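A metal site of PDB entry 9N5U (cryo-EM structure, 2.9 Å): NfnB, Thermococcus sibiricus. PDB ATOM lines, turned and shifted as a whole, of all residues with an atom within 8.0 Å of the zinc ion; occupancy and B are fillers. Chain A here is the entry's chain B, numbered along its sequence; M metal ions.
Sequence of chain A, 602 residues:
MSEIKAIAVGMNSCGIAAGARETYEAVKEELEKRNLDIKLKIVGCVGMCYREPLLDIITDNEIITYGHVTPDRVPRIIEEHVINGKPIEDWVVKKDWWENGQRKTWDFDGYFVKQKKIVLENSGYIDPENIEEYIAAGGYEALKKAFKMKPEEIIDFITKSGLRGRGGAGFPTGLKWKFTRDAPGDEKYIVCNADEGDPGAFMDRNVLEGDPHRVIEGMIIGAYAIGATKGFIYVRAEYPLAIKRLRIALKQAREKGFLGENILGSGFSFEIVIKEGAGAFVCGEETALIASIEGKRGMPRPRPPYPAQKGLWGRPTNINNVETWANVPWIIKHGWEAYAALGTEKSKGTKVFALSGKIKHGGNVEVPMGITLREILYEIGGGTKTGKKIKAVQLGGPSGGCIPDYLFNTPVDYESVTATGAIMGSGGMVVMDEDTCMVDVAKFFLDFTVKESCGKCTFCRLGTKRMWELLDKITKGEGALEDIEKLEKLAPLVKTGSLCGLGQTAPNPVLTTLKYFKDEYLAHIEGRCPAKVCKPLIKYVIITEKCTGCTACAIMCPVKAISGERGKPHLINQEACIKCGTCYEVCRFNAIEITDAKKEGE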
ATOM      1  N   THR A 436     -12.205  20.703 -33.034  1.00  0.00           N
ATOM      2  CA  THR A 436     -11.351  20.700 -31.853  1.00  0.00           C
ATOM      3  C   THR A 436     -11.770  21.817 -30.906  1.00  0.00           C
ATOM      4  O   THR A 436     -11.889  22.979 -31.322  1.00  0.00           O
ATOM      5  CB  THR A 436      -9.883  20.878 -32.254  1.00  0.00           C
ATOM      6  OG1 THR A 436      -9.454  19.738 -33.004  1.00  0.00           O
ATOM      7  CG2 THR A 436      -9.007  21.011 -31.016  1.00  0.00           C
ATOM      8  N   CYS A 437     -12.008  21.460 -29.649  1.00  0.00           N
ATOM      9  CA  CYS A 437     -12.316  22.430 -28.606  1.00  0.00           C
ATOM     10  C   CYS A 437     -11.005  22.940 -28.027  1.00  0.00           C
ATOM     11  O   CYS A 437     -10.171  22.150 -27.578  1.00  0.00           O
ATOM     12  CB  CYS A 437     -13.184  21.786 -27.534  1.00  0.00           C
ATOM     13  SG  CYS A 437     -13.423  22.725 -26.017  1.00  0.00           S
ATOM     14  N   MET A 438     -10.817  24.264 -28.057  1.00  0.00           N
ATOM     15  CA  MET A 438      -9.566  24.833 -27.573  1.00  0.00           C
ATOM     16  C   MET A 438      -9.448  24.736 -26.059  1.00  0.00           C
ATOM     17  O   MET A 438      -8.337  24.627 -25.538  1.00  0.00           O
ATOM     18  CB  MET A 438      -9.450  26.288 -28.035  1.00  0.00           C
ATOM     19  CG  MET A 438      -9.645  26.484 -29.523  1.00  0.00           C
ATOM     20  SD  MET A 438      -8.725  25.298 -30.525  1.00  0.00           S
ATOM     21  CE  MET A 438      -7.041  25.695 -30.081  1.00  0.00           C
ATOM     22  N   VAL A 439     -10.581  24.766 -25.363  1.00  0.00           N
ATOM     23  CA  VAL A 439     -10.565  24.555 -23.918  1.00  0.00           C
ATOM     24  C   VAL A 439     -10.108  23.138 -23.594  1.00  0.00           C
ATOM     25  O   VAL A 439      -9.347  22.915 -22.660  1.00  0.00           O
ATOM     26  CB  VAL A 439     -11.954  24.857 -23.324  1.00  0.00           C
ATOM     27  CG1 VAL A 439     -11.866  25.122 -21.840  1.00  0.00           C
ATOM     28  CG2 VAL A 439     -12.580  26.040 -24.035  1.00  0.00           C
ATOM     29  N   ASP A 440     -10.547  22.161 -24.391  1.00  0.00           N
ATOM     30  CA  ASP A 440     -10.118  20.779 -24.207  1.00  0.00           C
ATOM     31  C   ASP A 440      -8.622  20.629 -24.460  1.00  0.00           C
ATOM     32  O   ASP A 440      -7.937  19.878 -23.763  1.00  0.00           O
ATOM     33  CB  ASP A 440     -10.926  19.856 -25.119  1.00  0.00           C
ATOM     34  CG  ASP A 440     -10.996  18.446 -24.598  1.00  0.00           C
ATOM     35  OD1 ASP A 440     -11.654  18.218 -23.561  1.00  0.00           O
ATOM     36  OD2 ASP A 440     -10.412  17.545 -25.237  1.00  0.00           O
ATOM     37  N   VAL A 441      -8.098  21.340 -25.463  1.00  0.00           N
ATOM     38  CA  VAL A 441      -6.674  21.290 -25.757  1.00  0.00           C
ATOM     39  C   VAL A 441      -5.864  21.894 -24.608  1.00  0.00           C
ATOM     40  O   VAL A 441      -4.843  21.319 -24.175  1.00  0.00           O
ATOM     41  CB  VAL A 441      -6.393  21.993 -27.094  1.00  0.00           C
ATOM     42  CG1 VAL A 441      -4.975  22.494 -27.165  1.00  0.00           C
ATOM     43  CG2 VAL A 441      -6.667  21.036 -28.227  1.00  0.00           C
ATOM     44  N   ILE A 474     -14.528  24.587 -15.986  1.00  0.00           N
ATOM     45  CA  ILE A 474     -15.110  25.256 -17.153  1.00  0.00           C
ATOM     46  C   ILE A 474     -15.618  24.224 -18.157  1.00  0.00           C
ATOM     47  O   ILE A 474     -16.685  24.405 -18.766  1.00  0.00           O
ATOM     48  CB  ILE A 474     -14.086  26.217 -17.785  1.00  0.00           C
ATOM     49  CG1 ILE A 474     -13.743  27.336 -16.809  1.00  0.00           C
ATOM     50  CG2 ILE A 474     -14.618  26.807 -19.067  1.00  0.00           C
ATOM     51  CD1 ILE A 474     -12.692  28.281 -17.330  1.00  0.00           C
ATOM     52  N   THR A 475     -14.868  23.136 -18.346  1.00  0.00           N
ATOM     53  CA  THR A 475     -15.239  22.121 -19.317  1.00  0.00           C
ATOM     54  C   THR A 475     -16.521  21.397 -18.919  1.00  0.00           C
ATOM     55  O   THR A 475     -17.351  21.082 -19.782  1.00  0.00           O
ATOM     56  CB  THR A 475     -14.076  21.143 -19.504  1.00  0.00           C
ATOM     57  OG1 THR A 475     -13.019  21.794 -20.210  1.00  0.00           O
ATOM     58  CG2 THR A 475     -14.499  19.904 -20.269  1.00  0.00           C
ATOM     59  N   LYS A 476     -16.707  21.132 -17.635  1.00  0.00           N
ATOM     60  CA  LYS A 476     -17.904  20.443 -17.167  1.00  0.00           C
ATOM     61  C   LYS A 476     -19.147  21.327 -17.183  1.00  0.00           C
ATOM     62  O   LYS A 476     -20.249  20.826 -16.946  1.00  0.00           O
ATOM     63  CB  LYS A 476     -17.674  19.882 -15.761  1.00  0.00           C
ATOM     64  CG  LYS A 476     -16.708  18.713 -15.745  1.00  0.00           C
ATOM     65  CD  LYS A 476     -16.054  18.535 -14.391  1.00  0.00           C
ATOM     66  CE  LYS A 476     -17.073  18.292 -13.308  1.00  0.00           C
ATOM     67  NZ  LYS A 476     -16.426  18.115 -11.982  1.00  0.00           N
ATOM     68  N   GLU A 520     -14.679  30.838 -27.286  1.00  0.00           N
ATOM     69  CA  GLU A 520     -14.966  29.457 -26.887  1.00  0.00           C
ATOM     70  C   GLU A 520     -15.087  29.335 -25.375  1.00  0.00           C
ATOM     71  O   GLU A 520     -15.958  28.607 -24.875  1.00  0.00           O
ATOM     72  CB  GLU A 520     -13.888  28.519 -27.418  1.00  0.00           C
ATOM     73  CG  GLU A 520     -13.859  28.426 -28.934  1.00  0.00           C
ATOM     74  CD  GLU A 520     -13.220  27.151 -29.410  1.00  0.00           C
ATOM     75  OE1 GLU A 520     -12.948  26.275 -28.560  1.00  0.00           O
ATOM     76  OE2 GLU A 520     -13.011  27.007 -30.630  1.00  0.00           O
ATOM     77  N   TYR A 521     -14.219  30.023 -24.636  1.00  0.00           N
ATOM     78  CA  TYR A 521     -14.329  30.028 -23.176  1.00  0.00           C
ATOM     79  C   TYR A 521     -15.667  30.593 -22.729  1.00  0.00           C
ATOM     80  O   TYR A 521     -16.353  29.996 -21.888  1.00  0.00           O
ATOM     81  CB  TYR A 521     -13.181  30.849 -22.580  1.00  0.00           C
ATOM     82  CG  TYR A 521     -11.861  30.139 -22.488  1.00  0.00           C
ATOM     83  CD1 TYR A 521     -11.080  29.944 -23.615  1.00  0.00           C
ATOM     84  CD2 TYR A 521     -11.389  29.664 -21.279  1.00  0.00           C
ATOM     85  CE1 TYR A 521      -9.878  29.288 -23.541  1.00  0.00           C
ATOM     86  CE2 TYR A 521     -10.184  29.008 -21.192  1.00  0.00           C
ATOM     87  CZ  TYR A 521      -9.428  28.819 -22.334  1.00  0.00           C
ATOM     88  OH  TYR A 521      -8.220  28.173 -22.248  1.00  0.00           O
ATOM     89  N   ALA A 523     -18.387  30.729 -24.403  1.00  0.00           N
ATOM     90  CA  ALA A 523     -19.448  29.804 -24.763  1.00  0.00           C
ATOM     91  C   ALA A 523     -19.517  28.620 -23.814  1.00  0.00           C
ATOM     92  O   ALA A 523     -20.596  28.070 -23.575  1.00  0.00           O
ATOM     93  CB  ALA A 523     -19.246  29.324 -26.201  1.00  0.00           C
ATOM     94  N   HIS A 524     -18.367  28.211 -23.253  1.00  0.00           N
ATOM     95  CA  HIS A 524     -18.380  27.152 -22.249  1.00  0.00           C
ATOM     96  C   HIS A 524     -18.952  27.633 -20.925  1.00  0.00           C
ATOM     97  O   HIS A 524     -19.480  26.825 -20.154  1.00  0.00           O
ATOM     98  CB  HIS A 524     -16.978  26.587 -22.059  1.00  0.00           C
ATOM     99  CG  HIS A 524     -16.543  25.688 -23.171  1.00  0.00           C
ATOM    100  ND1 HIS A 524     -16.211  26.143 -24.428  1.00  0.00           N
ATOM    101  CD2 HIS A 524     -16.397  24.341 -23.215  1.00  0.00           C
ATOM    102  CE1 HIS A 524     -15.886  25.126 -25.195  1.00  0.00           C
ATOM    103  NE2 HIS A 524     -15.984  24.017 -24.490  1.00  0.00           N
ATOM    104  N   ARG A 528     -22.172  25.393 -23.431  1.00  0.00           N
ATOM    105  CA  ARG A 528     -22.193  24.911 -24.811  1.00  0.00           C
ATOM    106  C   ARG A 528     -20.771  24.776 -25.316  1.00  0.00           C
ATOM    107  O   ARG A 528     -19.916  25.615 -25.041  1.00  0.00           O
ATOM    108  CB  ARG A 528     -23.000  25.866 -25.685  1.00  0.00           C
ATOM    109  CG  ARG A 528     -22.920  25.605 -27.174  1.00  0.00           C
ATOM    110  CD  ARG A 528     -23.618  26.717 -27.951  1.00  0.00           C
ATOM    111  NE  ARG A 528     -22.962  28.013 -27.762  1.00  0.00           N
ATOM    112  CZ  ARG A 528     -23.414  28.957 -26.949  1.00  0.00           C
ATOM    113  NH1 ARG A 528     -24.510  28.791 -26.229  1.00  0.00           N
ATOM    114  NH2 ARG A 528     -22.740  30.102 -26.851  1.00  0.00           N
ATOM    115  N   CYS A 529     -20.504  23.695 -26.050  1.00  0.00           N
ATOM    116  CA  CYS A 529     -19.215  23.491 -26.676  1.00  0.00           C
ATOM    117  C   CYS A 529     -19.331  23.747 -28.174  1.00  0.00           C
ATOM    118  O   CYS A 529     -19.994  22.972 -28.875  1.00  0.00           O
ATOM    119  CB  CYS A 529     -18.695  22.069 -26.422  1.00  0.00           C
ATOM    120  SG  CYS A 529     -17.044  21.758 -27.062  1.00  0.00           S
ATOM    121  N   PRO A 530     -18.727  24.812 -28.694  1.00  0.00           N
ATOM    122  CA  PRO A 530     -18.849  25.108 -30.124  1.00  0.00           C
ATOM    123  C   PRO A 530     -18.249  24.047 -31.037  1.00  0.00           C
ATOM    124  O   PRO A 530     -18.576  24.021 -32.223  1.00  0.00           O
ATOM    125  CB  PRO A 530     -18.114  26.448 -30.277  1.00  0.00           C
ATOM    126  CG  PRO A 530     -18.168  27.054 -28.922  1.00  0.00           C
ATOM    127  CD  PRO A 530     -18.053  25.911 -27.968  1.00  0.00           C
ATOM    128  N   ALA A 531     -17.376  23.179 -30.523  1.00  0.00           N
ATOM    129  CA  ALA A 531     -16.821  22.082 -31.311  1.00  0.00           C
ATOM    130  C   ALA A 531     -17.464  20.743 -30.994  1.00  0.00           C
ATOM    131  O   ALA A 531     -17.126  19.744 -31.655  1.00  0.00           O
ATOM    132  CB  ALA A 531     -15.314  21.991 -31.098  1.00  0.00           C
ATOM    133  N   LYS A 532     -18.368  20.686 -30.015  1.00  0.00           N
ATOM    134  CA  LYS A 532     -19.048  19.462 -29.609  1.00  0.00           C
ATOM    135  C   LYS A 532     -18.050  18.379 -29.193  1.00  0.00           C
ATOM    136  O   LYS A 532     -18.094  17.241 -29.659  1.00  0.00           O
ATOM    137  CB  LYS A 532     -19.983  18.944 -30.695  1.00  0.00           C
ATOM    138  CG  LYS A 532     -20.862  20.010 -31.322  1.00  0.00           C
ATOM    139  CD  LYS A 532     -21.814  20.609 -30.310  1.00  0.00           C
ATOM    140  CE  LYS A 532     -22.449  21.874 -30.873  1.00  0.00           C
ATOM    141  NZ  LYS A 532     -23.055  21.641 -32.209  1.00  0.00           N
ATOM    142  N   VAL A 533     -17.145  18.741 -28.279  1.00  0.00           N
ATOM    143  CA  VAL A 533     -16.130  17.830 -27.784  1.00  0.00           C
ATOM    144  C   VAL A 533     -16.383  17.446 -26.331  1.00  0.00           C
ATOM    145  O   VAL A 533     -16.269  16.269 -25.972  1.00  0.00           O
ATOM    146  CB  VAL A 533     -14.716  18.425 -27.952  1.00  0.00           C
ATOM    147  CG1 VAL A 533     -13.670  17.493 -27.377  1.00  0.00           C
ATOM    148  CG2 VAL A 533     -14.434  18.716 -29.411  1.00  0.00           C
ATOM    149  N   CYS A 534     -16.718  18.412 -25.485  1.00  0.00           N
ATOM    150  CA  CYS A 534     -16.869  18.153 -24.058  1.00  0.00           C
ATOM    151  C   CYS A 534     -18.051  17.227 -23.808  1.00  0.00           C
ATOM    152  O   CYS A 534     -19.149  17.447 -24.328  1.00  0.00           O
ATOM    153  CB  CYS A 534     -17.055  19.474 -23.309  1.00  0.00           C
ATOM    154  SG  CYS A 534     -15.738  20.680 -23.620  1.00  0.00           S
ATOM    155  N   LYS A 535     -17.820  16.179 -23.016  1.00  0.00           N
ATOM    156  CA  LYS A 535     -18.860  15.178 -22.776  1.00  0.00           C
ATOM    157  C   LYS A 535     -20.099  15.732 -22.078  1.00  0.00           C
ATOM    158  O   LYS A 535     -21.210  15.487 -22.574  1.00  0.00           O
ATOM    159  CB  LYS A 535     -18.270  13.992 -22.003  1.00  0.00           C
ATOM    160  CG  LYS A 535     -17.174  13.257 -22.729  1.00  0.00           C
ATOM    161  CD  LYS A 535     -17.699  12.601 -23.981  1.00  0.00           C
ATOM    162  CE  LYS A 535     -16.662  11.669 -24.559  1.00  0.00           C
ATOM    163  NZ  LYS A 535     -16.273  10.629 -23.570  1.00  0.00           N
ATOM    164  N   LEU A 537     -21.303  18.714 -21.954  1.00  0.00           N
ATOM    165  CA  LEU A 537     -21.925  19.812 -22.664  1.00  0.00           C
ATOM    166  C   LEU A 537     -22.534  19.402 -24.001  1.00  0.00           C
ATOM    167  O   LEU A 537     -23.102  20.254 -24.698  1.00  0.00           O
ATOM    168  CB  LEU A 537     -20.907  20.937 -22.878  1.00  0.00           C
ATOM    169  CG  LEU A 537     -20.290  21.527 -21.607  1.00  0.00           C
ATOM    170  CD1 LEU A 537     -19.359  22.663 -21.951  1.00  0.00           C
ATOM    171  CD2 LEU A 537     -21.375  21.989 -20.664  1.00  0.00           C
ATOM    172  N   ILE A 538     -22.429  18.134 -24.389  1.00  0.00           N
ATOM    173  CA  ILE A 538     -23.027  17.638 -25.616  1.00  0.00           C
ATOM    174  C   ILE A 538     -24.098  16.616 -25.271  1.00  0.00           C
ATOM    175  O   ILE A 538     -23.974  15.873 -24.279  1.00  0.00           O
ATOM    176  CB  ILE A 538     -21.981  17.018 -26.574  1.00  0.00           C
ATOM    177  CG1 ILE A 538     -21.360  15.763 -25.962  1.00  0.00           C
ATOM    178  CG2 ILE A 538     -20.922  18.035 -26.900  1.00  0.00           C
ATOM    179  CD1 ILE A 538     -20.479  14.992 -26.920  1.00  0.00           C
HETATM  180 ZN    ZN M   1     -15.575  22.212 -25.342  1.00  0.00          ZN
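Within 4 Å of the zinc ion: Cys 437, His 524, Cys 529 and Cys 534. Along chain A the residues within 4 Å of the zinc ion span positions 437 to 534. The nearest printed residue that does not touch the zinc ion is Val 533 (4.7 Å).
NE2 of His 524 is bound to the zinc ion (2.0 Å). The side-chain sulfur (SG) of Cys 529 is bound to the zinc ion, at 2.3 Å. The zinc ion is bound by SG of Cys 534. SG of Cys 437 is bound to the zinc ion (2.3 Å). The zinc ion has four donor atoms within binding distance.
The side-chain sulfur of Cys 437 sits close to the backbone NH of Val 439, 3.6 Å away. The side-chain sulfur (SG) of Cys 529 lies close to the backbone NH (N) of Val 533 (3.3 Å). The side-chain sulfur (SG) of Cys 437 sits close to the backbone NH (N) of Asp 440, 3.4 Å away. SG of Cys 529 sits close to N of Lys 532 (3.4 Å). O of Glu 520 is in hydrogen-bond range of ND1 of His 524. The side-chain sulfur (SG) of Cys 529 sits close to the backbone NH (N) of Ala 531.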
